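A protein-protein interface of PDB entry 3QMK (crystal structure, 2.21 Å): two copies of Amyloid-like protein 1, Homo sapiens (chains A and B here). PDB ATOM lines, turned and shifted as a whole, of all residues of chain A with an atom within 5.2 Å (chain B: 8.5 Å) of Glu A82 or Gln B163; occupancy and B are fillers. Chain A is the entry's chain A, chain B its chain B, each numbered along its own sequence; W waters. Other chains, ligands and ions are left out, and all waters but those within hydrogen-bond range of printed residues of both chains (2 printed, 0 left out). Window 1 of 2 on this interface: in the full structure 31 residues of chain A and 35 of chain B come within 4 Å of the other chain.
Water W2 bridges the side-chain carboxylate of Glu A82 (2.6 Å) and the backbone carbonyl oxygen of Pro B159 (2.7 Å).
Water W1 lies within hydrogen-bond range of OE1 of Gln B163, NH1 of Arg B166 and OE1 of Gln A79.
Of the 10 printed residues of chain A, 5 touch a printed residue of chain B.
Printed residues of chain A that touch a printed residue of chain B: Leu A78, Gln A79, Glu A82, Val A85 and Ser A86.
Hydrophobic or aromatic side chains of chain A that line the printed part of chain B: Leu A78 and Val A85.
Of the 18 printed residues of chain B, 8 touch a printed residue of chain A.
Hydrophobic or aromatic side chains of chain B within 4 Å of the printed part of chain A: Tyr B151, Ala B156 and Pro B159.
The side-chain amide oxygen of Gln B163 lies within hydrogen-bond range of the side-chain amide nitrogen of Gln A79, 2.6 Å away.
NE of Arg B166 lies within salt-bridge range of OE2 of Glu A82, 2.7 Å away.
The side-chain hydroxyl of Tyr B151 is in hydrogen-bond range of the side-chain carboxylate of Glu A82 (2.5 Å).
Among the printed residues, pairs that only touch across the chains: Ser A86 with Pro B159 (2.9 Å), Ser A86 with Ala B155 (3.3 Å), Gln A79 with Arg B166 (3.6 Å), Val A85 with Ala B156 (3.6 Å), Leu A78 with Arg B166 (3.7 Å), Glu A82 with Gln B163 (3.7 Å), Glu A82 with Ala B162 (3.8 Å), Val A85 with Gln B152 (3.8 Å), Leu A78 with Tyr B151 (3.9 Å), Glu A82 with Ala B155 (3.9 Å) and Ser A86 with Ala B156 (3.99 Å).
No position is printed for both chains.
Of the 14 pairs that touch across the chains among the printed residues, none has its exchanged pair printed and touching as well.
Glu A82 touches just these residues of chain B: Tyr B151, Ala B155, Ala B162, Gln B163 and Arg B166.
Of chain A, only Gln A79 and Glu A82 come within 4 Å of Gln B163.
Of the printed residues of chain B, Gln A79 touches Gln B163 and Arg B166.
Of the printed residues of chain A, Ala B162 touches Glu A82.
Printed residues of chain A within 4 Å of Arg B166: Leu A78 (3.7 Å), Gln A79 (3.6 Å) and Glu A82 (2.7 Å).
Thr A80 touches none of the printed residues of chain B.
Asp B158 touches none of the printed residues of chain A.
The nearest residue of chain B that does not touch Glu A82 is Pro B159 (4.2 Å).
The nearest printed residue of chain A that does not touch Gln B163 is Glu A83 (6.8 Å).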
ATOM      1  N   LEU A  78       3.075   8.468   3.805  1.00  0.00           N
ATOM      2  CA  LEU A  78       1.968   9.414   3.687  1.00  0.00           C
ATOM      3  C   LEU A  78       0.607   8.722   3.883  1.00  0.00           C
ATOM      4  O   LEU A  78      -0.317   9.299   4.461  1.00  0.00           O
ATOM      5  CB  LEU A  78       2.055  10.164   2.338  1.00  0.00           C
ATOM      6  CG  LEU A  78       3.227  11.171   2.308  1.00  0.00           C
ATOM      7  CD1 LEU A  78       3.333  11.875   0.967  1.00  0.00           C
ATOM      8  CD2 LEU A  78       3.043  12.196   3.415  1.00  0.00           C
ATOM      9  N   GLN A  79       0.499   7.477   3.433  1.00  0.00           N
ATOM     10  CA  GLN A  79      -0.732   6.707   3.590  1.00  0.00           C
ATOM     11  C   GLN A  79      -1.090   6.666   5.074  1.00  0.00           C
ATOM     12  O   GLN A  79      -2.204   6.991   5.476  1.00  0.00           O
ATOM     13  CB  GLN A  79      -0.524   5.274   3.105  1.00  0.00           C
ATOM     14  CG  GLN A  79      -1.762   4.402   3.210  1.00  0.00           C
ATOM     15  CD  GLN A  79      -2.436   4.200   1.872  1.00  0.00           C
ATOM     16  OE1 GLN A  79      -1.881   3.558   0.981  1.00  0.00           O
ATOM     17  NE2 GLN A  79      -3.635   4.750   1.716  1.00  0.00           N
ATOM     18  N   THR A  80      -0.117   6.245   5.870  1.00  0.00           N
ATOM     19  CA  THR A  80      -0.239   6.126   7.310  1.00  0.00           C
ATOM     20  C   THR A  80      -0.575   7.477   7.948  1.00  0.00           C
ATOM     21  O   THR A  80      -1.440   7.571   8.815  1.00  0.00           O
ATOM     22  CB  THR A  80       1.083   5.605   7.912  1.00  0.00           C
ATOM     23  OG1 THR A  80       1.420   4.345   7.316  1.00  0.00           O
ATOM     24  CG2 THR A  80       0.953   5.439   9.413  1.00  0.00           C
ATOM     25  N   LEU A  81       0.116   8.527   7.511  1.00  0.00           N
ATOM     26  CA  LEU A  81      -0.116   9.862   8.046  1.00  0.00           C
ATOM     27  C   LEU A  81      -1.552  10.289   7.732  1.00  0.00           C
ATOM     28  O   LEU A  81      -2.245  10.827   8.594  1.00  0.00           O
ATOM     29  CB  LEU A  81       0.886  10.840   7.442  1.00  0.00           C
ATOM     30  CG  LEU A  81       1.010  12.212   8.108  1.00  0.00           C
ATOM     31  CD1 LEU A  81       1.140  12.063   9.621  1.00  0.00           C
ATOM     32  CD2 LEU A  81       2.236  12.928   7.540  1.00  0.00           C
ATOM     33  N   GLU A  82      -1.997  10.041   6.503  1.00  0.00           N
ATOM     34  CA  GLU A  82      -3.357  10.386   6.104  1.00  0.00           C
ATOM     35  C   GLU A  82      -4.375   9.654   6.997  1.00  0.00           C
ATOM     36  O   GLU A  82      -5.408  10.213   7.372  1.00  0.00           O
ATOM     37  CB  GLU A  82      -3.594   9.998   4.640  1.00  0.00           C
ATOM     38  CG  GLU A  82      -2.784  10.828   3.644  1.00  0.00           C
ATOM     39  CD  GLU A  82      -2.655  10.174   2.253  1.00  0.00           C
ATOM     40  OE1 GLU A  82      -3.336   9.160   1.994  1.00  0.00           O
ATOM     41  OE2 GLU A  82      -1.868  10.692   1.413  1.00  0.00           O
ATOM     42  N   GLU A  83      -4.068   8.405   7.344  1.00  0.00           N
ATOM     43  CA  GLU A  83      -4.962   7.606   8.167  1.00  0.00           C
ATOM     44  C   GLU A  83      -4.955   8.102   9.608  1.00  0.00           C
ATOM     45  O   GLU A  83      -5.947   7.965  10.322  1.00  0.00           O
ATOM     46  CB  GLU A  83      -4.564   6.128   8.120  1.00  0.00           C
ATOM     47  CG  GLU A  83      -4.617   5.493   6.724  1.00  0.00           C
ATOM     48  CD  GLU A  83      -3.995   4.094   6.690  1.00  0.00           C
ATOM     49  OE1 GLU A  83      -3.200   3.775   7.605  1.00  0.00           O
ATOM     50  OE2 GLU A  83      -4.288   3.326   5.743  1.00  0.00           O
ATOM     51  N   GLN A  84      -3.834   8.677  10.024  1.00  0.00           N
ATOM     52  CA  GLN A  84      -3.712   9.210  11.368  1.00  0.00           C
ATOM     53  C   GLN A  84      -4.539  10.479  11.449  1.00  0.00           C
ATOM     54  O   GLN A  84      -5.243  10.711  12.424  1.00  0.00           O
ATOM     55  CB  GLN A  84      -2.258   9.554  11.686  1.00  0.00           C
ATOM     56  CG  GLN A  84      -1.395   8.392  12.122  1.00  0.00           C
ATOM     57  CD  GLN A  84       0.051   8.816  12.329  1.00  0.00           C
ATOM     58  OE1 GLN A  84       0.326   9.813  13.001  1.00  0.00           O
ATOM     59  NE2 GLN A  84       0.985   8.059  11.755  1.00  0.00           N
ATOM     60  N   VAL A  85      -4.430  11.303  10.410  1.00  0.00           N
ATOM     61  CA  VAL A  85      -5.160  12.561  10.336  1.00  0.00           C
ATOM     62  C   VAL A  85      -6.656  12.314  10.271  1.00  0.00           C
ATOM     63  O   VAL A  85      -7.437  13.013  10.910  1.00  0.00           O
ATOM     64  CB  VAL A  85      -4.721  13.371   9.105  1.00  0.00           C
ATOM     65  CG1 VAL A  85      -5.651  14.581   8.883  1.00  0.00           C
ATOM     66  CG2 VAL A  85      -3.284  13.827   9.316  1.00  0.00           C
ATOM     67  N   SER A  86      -7.050  11.308   9.500  1.00  0.00           N
ATOM     68  CA  SER A  86      -8.463  10.954   9.371  1.00  0.00           C
ATOM     69  C   SER A  86      -9.016  10.404  10.707  1.00  0.00           C
ATOM     70  O   SER A  86     -10.090  10.800  11.134  1.00  0.00           O
ATOM     71  CB  SER A  86      -8.642   9.922   8.259  1.00  0.00           C
ATOM     72  OG  SER A  86      -9.999   9.580   8.107  1.00  0.00           O
ATOM     73  N   GLY A  87      -8.266   9.511  11.362  1.00  0.00           N
ATOM     74  CA  GLY A  87      -8.693   8.933  12.635  1.00  0.00           C
ATOM     75  C   GLY A  87      -8.777   9.962  13.761  1.00  0.00           C
ATOM     76  O   GLY A  87      -9.723   9.978  14.540  1.00  0.00           O
ATOM     77  N   TYR B 151      -4.338  19.875   1.389  1.00  0.00           N
ATOM     78  CA  TYR B 151      -4.053  18.438   1.404  1.00  0.00           C
ATOM     79  C   TYR B 151      -4.437  17.866   2.791  1.00  0.00           C
ATOM     80  O   TYR B 151      -5.133  16.860   2.886  1.00  0.00           O
ATOM     81  CB  TYR B 151      -2.558  18.181   1.095  1.00  0.00           C
ATOM     82  CG  TYR B 151      -2.098  16.743   1.278  1.00  0.00           C
ATOM     83  CD1 TYR B 151      -2.760  15.676   0.652  1.00  0.00           C
ATOM     84  CD2 TYR B 151      -0.981  16.450   2.065  1.00  0.00           C
ATOM     85  CE1 TYR B 151      -2.312  14.352   0.811  1.00  0.00           C
ATOM     86  CE2 TYR B 151      -0.521  15.136   2.232  1.00  0.00           C
ATOM     87  CZ  TYR B 151      -1.185  14.096   1.605  1.00  0.00           C
ATOM     88  OH  TYR B 151      -0.694  12.815   1.764  1.00  0.00           O
ATOM     89  N   GLN B 152      -3.992  18.526   3.858  1.00  0.00           N
ATOM     90  CA  GLN B 152      -4.293  18.086   5.218  1.00  0.00           C
ATOM     91  C   GLN B 152      -5.806  18.012   5.472  1.00  0.00           C
ATOM     92  O   GLN B 152      -6.293  17.067   6.111  1.00  0.00           O
ATOM     93  CB  GLN B 152      -3.612  19.010   6.244  1.00  0.00           C
ATOM     94  CG  GLN B 152      -4.147  18.890   7.673  1.00  0.00           C
ATOM     95  CD  GLN B 152      -5.395  19.747   7.904  1.00  0.00           C
ATOM     96  OE1 GLN B 152      -6.199  19.469   8.802  1.00  0.00           O
ATOM     97  NE2 GLN B 152      -5.551  20.800   7.104  1.00  0.00           N
ATOM     98  N   VAL B 154      -8.248  17.564   3.173  1.00  0.00           N
ATOM     99  CA  VAL B 154      -8.839  16.458   2.428  1.00  0.00           C
ATOM    100  C   VAL B 154      -8.582  15.111   3.138  1.00  0.00           C
ATOM    101  O   VAL B 154      -9.432  14.224   3.104  1.00  0.00           O
ATOM    102  CB  VAL B 154      -8.280  16.393   0.978  1.00  0.00           C
ATOM    103  CG1 VAL B 154      -8.790  15.153   0.269  1.00  0.00           C
ATOM    104  CG2 VAL B 154      -8.698  17.635   0.205  1.00  0.00           C
ATOM    105  N   ALA B 155      -7.418  14.951   3.770  1.00  0.00           N
ATOM    106  CA  ALA B 155      -7.114  13.700   4.477  1.00  0.00           C
ATOM    107  C   ALA B 155      -7.957  13.581   5.746  1.00  0.00           C
ATOM    108  O   ALA B 155      -8.335  12.479   6.159  1.00  0.00           O
ATOM    109  CB  ALA B 155      -5.639  13.633   4.849  1.00  0.00           C
ATOM    110  N   ALA B 156      -8.231  14.725   6.367  1.00  0.00           N
ATOM    111  CA  ALA B 156      -9.007  14.777   7.591  1.00  0.00           C
ATOM    112  C   ALA B 156     -10.452  14.356   7.382  1.00  0.00           C
ATOM    113  O   ALA B 156     -11.063  13.774   8.276  1.00  0.00           O
ATOM    114  CB  ALA B 156      -8.962  16.181   8.179  1.00  0.00           C
ATOM    115  N   VAL B 157     -10.995  14.633   6.199  1.00  0.00           N
ATOM    116  CA  VAL B 157     -12.387  14.311   5.927  1.00  0.00           C
ATOM    117  C   VAL B 157     -12.670  13.334   4.781  1.00  0.00           C
ATOM    118  O   VAL B 157     -13.771  12.794   4.696  1.00  0.00           O
ATOM    119  CB  VAL B 157     -13.213  15.615   5.670  1.00  0.00           C
ATOM    120  CG1 VAL B 157     -12.969  16.618   6.780  1.00  0.00           C
ATOM    121  CG2 VAL B 157     -12.840  16.233   4.327  1.00  0.00           C
ATOM    122  N   ASP B 158     -11.693  13.093   3.912  1.00  0.00           N
ATOM    123  CA  ASP B 158     -11.905  12.206   2.759  1.00  0.00           C
ATOM    124  C   ASP B 158     -10.576  11.544   2.380  1.00  0.00           C
ATOM    125  O   ASP B 158      -9.953  11.890   1.365  1.00  0.00           O
ATOM    126  CB  ASP B 158     -12.444  13.036   1.585  1.00  0.00           C
ATOM    127  CG  ASP B 158     -12.941  12.182   0.422  1.00  0.00           C
ATOM    128  OD1 ASP B 158     -12.596  10.983   0.345  1.00  0.00           O
ATOM    129  OD2 ASP B 158     -13.675  12.732  -0.432  1.00  0.00           O
ATOM    130  N   PRO B 159     -10.128  10.583   3.203  1.00  0.00           N
ATOM    131  CA  PRO B 159      -8.888   9.813   3.060  1.00  0.00           C
ATOM    132  C   PRO B 159      -8.589   9.239   1.674  1.00  0.00           C
ATOM    133  O   PRO B 159      -7.438   9.233   1.239  1.00  0.00           O
ATOM    134  CB  PRO B 159      -9.049   8.718   4.106  1.00  0.00           C
ATOM    135  CG  PRO B 159      -9.812   9.414   5.181  1.00  0.00           C
ATOM    136  CD  PRO B 159     -10.873  10.136   4.394  1.00  0.00           C
ATOM    137  N   GLU B 160      -9.613   8.746   0.989  1.00  0.00           N
ATOM    138  CA  GLU B 160      -9.403   8.148  -0.325  1.00  0.00           C
ATOM    139  C   GLU B 160      -8.984   9.182  -1.343  1.00  0.00           C
ATOM    140  O   GLU B 160      -8.134   8.914  -2.190  1.00  0.00           O
ATOM    141  CB  GLU B 160     -10.667   7.442  -0.798  1.00  0.00           C
ATOM    142  N   LYS B 161      -9.598  10.358  -1.262  1.00  0.00           N
ATOM    143  CA  LYS B 161      -9.288  11.435  -2.181  1.00  0.00           C
ATOM    144  C   LYS B 161      -7.893  11.981  -1.850  1.00  0.00           C
ATOM    145  O   LYS B 161      -7.163  12.424  -2.736  1.00  0.00           O
ATOM    146  CB  LYS B 161     -10.337  12.546  -2.102  1.00  0.00           C
ATOM    147  N   ALA B 162      -7.526  11.935  -0.571  1.00  0.00           N
ATOM    148  CA  ALA B 162      -6.218  12.408  -0.149  1.00  0.00           C
ATOM    149  C   ALA B 162      -5.168  11.536  -0.825  1.00  0.00           C
ATOM    150  O   ALA B 162      -4.135  12.027  -1.280  1.00  0.00           O
ATOM    151  CB  ALA B 162      -6.089  12.327   1.367  1.00  0.00           C
ATOM    152  N   GLN B 163      -5.441  10.236  -0.893  1.00  0.00           N
ATOM    153  CA  GLN B 163      -4.530   9.313  -1.549  1.00  0.00           C
ATOM    154  C   GLN B 163      -4.387   9.654  -3.032  1.00  0.00           C
ATOM    155  O   GLN B 163      -3.294   9.582  -3.589  1.00  0.00           O
ATOM    156  CB  GLN B 163      -5.019   7.876  -1.402  1.00  0.00           C
ATOM    157  CG  GLN B 163      -4.307   6.894  -2.315  1.00  0.00           C
ATOM    158  CD  GLN B 163      -4.589   5.456  -1.933  1.00  0.00           C
ATOM    159  OE1 GLN B 163      -4.171   4.989  -0.866  1.00  0.00           O
ATOM    160  NE2 GLN B 163      -5.309   4.745  -2.793  1.00  0.00           N
ATOM    161  N   GLN B 164      -5.491  10.036  -3.662  1.00  0.00           N
ATOM    162  CA  GLN B 164      -5.489  10.382  -5.087  1.00  0.00           C
ATOM    163  C   GLN B 164      -4.655  11.619  -5.443  1.00  0.00           C
ATOM    164  O   GLN B 164      -4.034  11.663  -6.503  1.00  0.00           O
ATOM    165  CB  GLN B 164      -6.922  10.615  -5.584  1.00  0.00           C
ATOM    166  CG  GLN B 164      -7.875   9.437  -5.374  1.00  0.00           C
ATOM    167  CD  GLN B 164      -9.309   9.732  -5.835  1.00  0.00           C
ATOM    168  OE1 GLN B 164      -9.937  10.696  -5.388  1.00  0.00           O
ATOM    169  NE2 GLN B 164      -9.829   8.892  -6.723  1.00  0.00           N
ATOM    170  N   MET B 165      -4.647  12.622  -4.568  1.00  0.00           N
ATOM    171  CA  MET B 165      -3.921  13.873  -4.830  1.00  0.00           C
ATOM    172  C   MET B 165      -2.476  13.913  -4.332  1.00  0.00           C
ATOM    173  O   MET B 165      -1.717  14.806  -4.688  1.00  0.00           O
ATOM    174  CB  MET B 165      -4.683  15.036  -4.197  1.00  0.00           C
ATOM    175  CG  MET B 165      -4.559  15.037  -2.690  1.00  0.00           C
ATOM    176  SD  MET B 165      -5.846  15.997  -1.869  1.00  0.00           S
ATOM    177  CE  MET B 165      -5.297  17.744  -2.161  1.00  0.00           C
ATOM    178  N   ARG B 166      -2.120  12.942  -3.508  1.00  0.00           N
ATOM    179  CA  ARG B 166      -0.803  12.845  -2.892  1.00  0.00           C
ATOM    180  C   ARG B 166       0.391  13.215  -3.799  1.00  0.00           C
ATOM    181  O   ARG B 166       1.181  14.114  -3.466  1.00  0.00           O
ATOM    182  CB  ARG B 166      -0.637  11.434  -2.329  1.00  0.00           C
ATOM    183  CG  ARG B 166       0.532  11.227  -1.399  1.00  0.00           C
ATOM    184  CD  ARG B 166       0.676   9.744  -1.091  1.00  0.00           C
ATOM    185  NE  ARG B 166      -0.489   9.206  -0.387  1.00  0.00           N
ATOM    186  CZ  ARG B 166      -0.881   7.937  -0.452  1.00  0.00           C
ATOM    187  NH1 ARG B 166      -0.201   7.068  -1.198  1.00  0.00           N
ATOM    188  NH2 ARG B 166      -1.945   7.529   0.238  1.00  0.00           N
ATOM    189  N   PHE B 167       0.520  12.528  -4.934  1.00  0.00           N
ATOM    190  CA  PHE B 167       1.608  12.782  -5.875  1.00  0.00           C
ATOM    191  C   PHE B 167       1.522  14.193  -6.479  1.00  0.00           C
ATOM    192  O   PHE B 167       2.538  14.845  -6.707  1.00  0.00           O
ATOM    193  CB  PHE B 167       1.588  11.741  -7.007  1.00  0.00           C
ATOM    194  CG  PHE B 167       2.812  11.783  -7.880  1.00  0.00           C
ATOM    195  CD1 PHE B 167       4.025  11.289  -7.410  1.00  0.00           C
ATOM    196  CD2 PHE B 167       2.771  12.377  -9.133  1.00  0.00           C
ATOM    197  CE1 PHE B 167       5.186  11.388  -8.170  1.00  0.00           C
ATOM    198  CE2 PHE B 167       3.937  12.484  -9.914  1.00  0.00           C
ATOM    199  CZ  PHE B 167       5.145  11.988  -9.423  1.00  0.00           C
ATOM    200  N   GLN B 168       0.301  14.657  -6.728  1.00  0.00           N
ATOM    201  CA  GLN B 168       0.088  15.975  -7.300  1.00  0.00           C
ATOM    202  C   GLN B 168       0.525  17.100  -6.318  1.00  0.00           C
ATOM    203  O   GLN B 168       1.039  18.131  -6.738  1.00  0.00           O
ATOM    204  CB  GLN B 168      -1.389  16.115  -7.698  1.00  0.00           C
ATOM    205  CG  GLN B 168      -1.751  17.395  -8.444  1.00  0.00           C
ATOM    206  CD  GLN B 168      -1.688  18.621  -7.558  1.00  0.00           C
ATOM    207  OE1 GLN B 168      -2.304  18.662  -6.488  1.00  0.00           O
ATOM    208  NE2 GLN B 168      -0.949  19.636  -8.001  1.00  0.00           N
ATOM    209  N   VAL B 169       0.315  16.885  -5.022  1.00  0.00           N
ATOM    210  CA  VAL B 169       0.702  17.852  -3.994  1.00  0.00           C
ATOM    211  C   VAL B 169       2.234  17.890  -3.953  1.00  0.00           C
ATOM    212  O   VAL B 169       2.847  18.948  -3.985  1.00  0.00           O
ATOM    213  CB  VAL B 169       0.140  17.440  -2.598  1.00  0.00           C
ATOM    214  CG1 VAL B 169       0.783  18.294  -1.488  1.00  0.00           C
ATOM    215  CG2 VAL B 169      -1.379  17.616  -2.575  1.00  0.00           C
HETATM  216  O   HOH W   1      -1.664   4.718  -1.995  1.00  0.00           O
HETATM  217  O   HOH W   2      -5.607   8.023   2.726  1.00  0.00           O
